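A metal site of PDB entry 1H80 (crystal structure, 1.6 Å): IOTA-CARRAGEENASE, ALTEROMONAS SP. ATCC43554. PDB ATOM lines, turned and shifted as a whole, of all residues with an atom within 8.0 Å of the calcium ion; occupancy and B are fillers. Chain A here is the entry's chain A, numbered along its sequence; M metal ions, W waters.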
ATOM      1  N   GLY A  29      29.560   3.648 -11.892  1.00  0.00           N
ATOM      2  CA  GLY A  29      28.167   3.333 -12.171  1.00  0.00           C
ATOM      3  C   GLY A  29      27.693   1.891 -12.257  1.00  0.00           C
ATOM      4  O   GLY A  29      26.670   1.637 -12.895  1.00  0.00           O
ATOM      5  N   ALA A  30      28.394   0.962 -11.638  1.00  0.00           N
ATOM      6  CA  ALA A  30      27.933  -0.425 -11.668  1.00  0.00           C
ATOM      7  C   ALA A  30      26.681  -0.437 -10.794  1.00  0.00           C
ATOM      8  O   ALA A  30      26.473   0.453  -9.973  1.00  0.00           O
ATOM      9  CB  ALA A  30      28.987  -1.350 -11.093  1.00  0.00           C
ATOM     10  N   ASN A  31      25.833  -1.452 -10.975  1.00  0.00           N
ATOM     11  CA  ASN A  31      24.613  -1.553 -10.177  1.00  0.00           C
ATOM     12  C   ASN A  31      24.534  -2.936  -9.542  1.00  0.00           C
ATOM     13  O   ASN A  31      24.342  -3.934 -10.235  1.00  0.00           O
ATOM     14  CB  ASN A  31      23.387  -1.329 -11.059  1.00  0.00           C
ATOM     15  CG  ASN A  31      22.120  -1.150 -10.257  1.00  0.00           C
ATOM     16  OD1 ASN A  31      21.907  -1.826  -9.251  1.00  0.00           O
ATOM     17  ND2 ASN A  31      21.254  -0.244 -10.700  1.00  0.00           N
ATOM     18  N   GLY A  32      24.680  -2.990  -8.223  1.00  0.00           N
ATOM     19  CA  GLY A  32      24.627  -4.261  -7.533  1.00  0.00           C
ATOM     20  C   GLY A  32      23.246  -4.593  -6.983  1.00  0.00           C
ATOM     21  O   GLY A  32      23.107  -5.475  -6.131  1.00  0.00           O
ATOM     22  N   ASN A  33      22.239  -3.880  -7.458  1.00  0.00           N
ATOM     23  CA  ASN A  33      20.870  -4.094  -7.000  1.00  0.00           C
ATOM     24  C   ASN A  33      19.962  -4.687  -8.072  1.00  0.00           C
ATOM     25  O   ASN A  33      18.791  -4.968  -7.821  1.00  0.00           O
ATOM     26  CB  ASN A  33      20.269  -2.767  -6.507  1.00  0.00           C
ATOM     27  CG  ASN A  33      20.874  -2.316  -5.196  1.00  0.00           C
ATOM     28  OD1 ASN A  33      20.799  -1.134  -4.838  1.00  0.00           O
ATOM     29  ND2 ASN A  33      21.450  -3.247  -4.447  1.00  0.00           N
ATOM     30  N   ASP A  34      20.498  -4.869  -9.272  1.00  0.00           N
ATOM     31  CA  ASP A  34      19.711  -5.444 -10.361  1.00  0.00           C
ATOM     32  C   ASP A  34      20.314  -6.741 -10.855  1.00  0.00           C
ATOM     33  O   ASP A  34      21.203  -7.320 -10.214  1.00  0.00           O
ATOM     34  CB  ASP A  34      19.605  -4.449 -11.526  1.00  0.00           C
ATOM     35  CG  ASP A  34      20.968  -4.055 -12.076  1.00  0.00           C
ATOM     36  OD1 ASP A  34      21.904  -4.882 -12.000  1.00  0.00           O
ATOM     37  OD2 ASP A  34      21.083  -2.926 -12.596  1.00  0.00           O
ATOM     38  N   THR A  35      19.834  -7.215 -12.002  1.00  0.00           N
ATOM     39  CA  THR A  35      20.338  -8.462 -12.565  1.00  0.00           C
ATOM     40  C   THR A  35      21.046  -8.194 -13.895  1.00  0.00           C
ATOM     41  O   THR A  35      21.297  -9.118 -14.664  1.00  0.00           O
ATOM     42  CB  THR A  35      19.195  -9.451 -12.817  1.00  0.00           C
ATOM     43  OG1 THR A  35      18.202  -8.835 -13.643  1.00  0.00           O
ATOM     44  CG2 THR A  35      18.556  -9.871 -11.495  1.00  0.00           C
ATOM     45  N   SER A  36      21.373  -6.934 -14.138  1.00  0.00           N
ATOM     46  CA  SER A  36      22.035  -6.524 -15.370  1.00  0.00           C
ATOM     47  C   SER A  36      23.560  -6.594 -15.311  1.00  0.00           C
ATOM     48  O   SER A  36      24.157  -6.430 -14.255  1.00  0.00           O
ATOM     49  CB  SER A  36      21.606  -5.097 -15.731  1.00  0.00           C
ATOM     50  OG  SER A  36      20.196  -5.014 -15.902  1.00  0.00           O
ATOM     51  N   ASP A  37      24.163  -6.812 -16.476  1.00  0.00           N
ATOM     52  CA  ASP A  37      25.610  -6.925 -16.628  1.00  0.00           C
ATOM     53  C   ASP A  37      26.376  -5.701 -16.122  1.00  0.00           C
ATOM     54  O   ASP A  37      26.030  -4.570 -16.423  1.00  0.00           O
ATOM     55  CB  ASP A  37      25.928  -7.182 -18.118  1.00  0.00           C
ATOM     56  CG  ASP A  37      27.407  -7.331 -18.399  1.00  0.00           C
ATOM     57  OD1 ASP A  37      28.119  -7.936 -17.577  1.00  0.00           O
ATOM     58  OD2 ASP A  37      27.844  -6.858 -19.470  1.00  0.00           O
ATOM     59  N   ASP A  38      27.432  -5.960 -15.352  1.00  0.00           N
ATOM     60  CA  ASP A  38      28.249  -4.896 -14.784  1.00  0.00           C
ATOM     61  C   ASP A  38      29.678  -4.937 -15.317  1.00  0.00           C
ATOM     62  O   ASP A  38      30.563  -4.239 -14.815  1.00  0.00           O
ATOM     63  CB  ASP A  38      28.262  -5.040 -13.258  1.00  0.00           C
ATOM     64  CG  ASP A  38      26.879  -4.995 -12.668  1.00  0.00           C
ATOM     65  OD1 ASP A  38      26.241  -3.934 -12.746  1.00  0.00           O
ATOM     66  OD2 ASP A  38      26.415  -6.030 -12.132  1.00  0.00           O
ATOM     67  N   SER A  39      29.901  -5.756 -16.341  1.00  0.00           N
ATOM     68  CA  SER A  39      31.223  -5.913 -16.920  1.00  0.00           C
ATOM     69  C   SER A  39      31.882  -4.638 -17.425  1.00  0.00           C
ATOM     70  O   SER A  39      33.059  -4.393 -17.156  1.00  0.00           O
ATOM     71  CB  SER A  39      31.167  -6.943 -18.055  1.00  0.00           C
ATOM     72  OG  SER A  39      30.750  -8.205 -17.576  1.00  0.00           O
ATOM     73  N   ALA A  41      31.323  -1.557 -16.542  1.00  0.00           N
ATOM     74  CA  ALA A  41      31.652  -0.689 -15.410  1.00  0.00           C
ATOM     75  C   ALA A  41      32.982  -1.132 -14.806  1.00  0.00           C
ATOM     76  O   ALA A  41      33.875  -0.321 -14.562  1.00  0.00           O
ATOM     77  CB  ALA A  41      30.556  -0.753 -14.364  1.00  0.00           C
ATOM     78  N   THR A  64      25.094  -7.432  -5.632  1.00  0.00           N
ATOM     79  CA  THR A  64      25.217  -8.562  -6.538  1.00  0.00           C
ATOM     80  C   THR A  64      25.612  -8.031  -7.900  1.00  0.00           C
ATOM     81  O   THR A  64      24.936  -7.174  -8.467  1.00  0.00           O
ATOM     82  CB  THR A  64      23.891  -9.336  -6.633  1.00  0.00           C
ATOM     83  OG1 THR A  64      23.578  -9.886  -5.342  1.00  0.00           O
ATOM     84  CG2 THR A  64      24.003 -10.461  -7.641  1.00  0.00           C
ATOM     85  N   TYR A  65      26.702  -8.558  -8.429  1.00  0.00           N
ATOM     86  CA  TYR A  65      27.212  -8.115  -9.716  1.00  0.00           C
ATOM     87  C   TYR A  65      27.325  -9.233 -10.718  1.00  0.00           C
ATOM     88  O   TYR A  65      27.569 -10.390 -10.353  1.00  0.00           O
ATOM     89  CB  TYR A  65      28.588  -7.493  -9.539  1.00  0.00           C
ATOM     90  CG  TYR A  65      28.594  -6.380  -8.532  1.00  0.00           C
ATOM     91  CD1 TYR A  65      28.255  -5.082  -8.900  1.00  0.00           C
ATOM     92  CD2 TYR A  65      28.874  -6.628  -7.193  1.00  0.00           C
ATOM     93  CE1 TYR A  65      28.200  -4.066  -7.968  1.00  0.00           C
ATOM     94  CE2 TYR A  65      28.825  -5.621  -6.253  1.00  0.00           C
ATOM     95  CZ  TYR A  65      28.484  -4.339  -6.648  1.00  0.00           C
ATOM     96  OH  TYR A  65      28.424  -3.336  -5.717  1.00  0.00           O
ATOM     97  N   HIS A  66      27.150  -8.883 -11.981  1.00  0.00           N
ATOM     98  CA  HIS A  66      27.272  -9.835 -13.064  1.00  0.00           C
ATOM     99  C   HIS A  66      28.462  -9.413 -13.916  1.00  0.00           C
ATOM    100  O   HIS A  66      28.483  -8.321 -14.492  1.00  0.00           O
ATOM    101  CB  HIS A  66      25.989  -9.856 -13.903  1.00  0.00           C
ATOM    102  CG  HIS A  66      24.829 -10.482 -13.198  1.00  0.00           C
ATOM    103  ND1 HIS A  66      24.133  -9.847 -12.182  1.00  0.00           N
ATOM    104  CD2 HIS A  66      24.274 -11.713 -13.318  1.00  0.00           C
ATOM    105  CE1 HIS A  66      23.203 -10.662 -11.714  1.00  0.00           C
ATOM    106  NE2 HIS A  66      23.267 -11.799 -12.385  1.00  0.00           N
ATOM    107  N   PHE A  67      29.459 -10.288 -13.978  1.00  0.00           N
ATOM    108  CA  PHE A  67      30.668 -10.020 -14.753  1.00  0.00           C
ATOM    109  C   PHE A  67      30.979 -11.199 -15.654  1.00  0.00           C
ATOM    110  O   PHE A  67      30.589 -12.333 -15.379  1.00  0.00           O
ATOM    111  CB  PHE A  67      31.904  -9.849 -13.852  1.00  0.00           C
ATOM    112  CG  PHE A  67      31.779  -8.772 -12.821  1.00  0.00           C
ATOM    113  CD1 PHE A  67      31.424  -7.477 -13.170  1.00  0.00           C
ATOM    114  CD2 PHE A  67      32.097  -9.037 -11.489  1.00  0.00           C
ATOM    115  CE1 PHE A  67      31.387  -6.460 -12.214  1.00  0.00           C
ATOM    116  CE2 PHE A  67      32.060  -8.043 -10.525  1.00  0.00           C
ATOM    117  CZ  PHE A  67      31.708  -6.748 -10.887  1.00  0.00           C
ATOM    118  N   THR A  89      27.844 -13.256 -16.055  1.00  0.00           N
ATOM    119  CA  THR A  89      26.870 -12.686 -16.968  1.00  0.00           C
ATOM    120  C   THR A  89      26.597 -13.731 -18.037  1.00  0.00           C
ATOM    121  O   THR A  89      27.527 -14.399 -18.503  1.00  0.00           O
ATOM    122  CB  THR A  89      27.412 -11.430 -17.656  1.00  0.00           C
ATOM    123  OG1 THR A  89      27.809 -10.489 -16.653  1.00  0.00           O
ATOM    124  CG2 THR A  89      26.348 -10.798 -18.537  1.00  0.00           C
HETATM  125 CA    CA M   1      24.227  -5.073 -12.291  1.00  0.00          CA
HETATM  126  O   HOH W   1      23.596  -3.354 -13.724  1.00  0.00           O
HETATM  127  O   HOH W   2      23.710  -7.018 -10.895  1.00  0.00           O
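Water W2 lies within hydrogen-bond range of O of Asp 34 (2.6 Å), O of Thr 64 (2.7 Å) and ND1 of His 66 (3.1 Å).
OD1 of Asn 31 sits at hydrogen-bond distance from N of Asn 33 (2.7 Å). N of Asp 38 is in hydrogen-bond range of O of His 66.
Water W1 binds the calcium ion (2.3 Å). The side-chain carboxylate (OD1) of Asp 34 binds the calcium ion (2.3 Å). The calcium ion is bound by the backbone carbonyl oxygen (O) of Asn 31. OD1 of Asp 38 binds the calcium ion, at 2.4 Å. The calcium ion is bound by the backbone carbonyl oxygen (O) of Ser 36 (2.4 Å). The calcium ion is bound by OD2 of Asp 38 (2.4 Å). The calcium ion is bound by water W2, 2.4 Å away.
Of the 17 residues printed, 4 come within 4 Å of the calcium ion. The nearest printed residue that does not touch the calcium ion is Thr 64 (4.4 Å).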
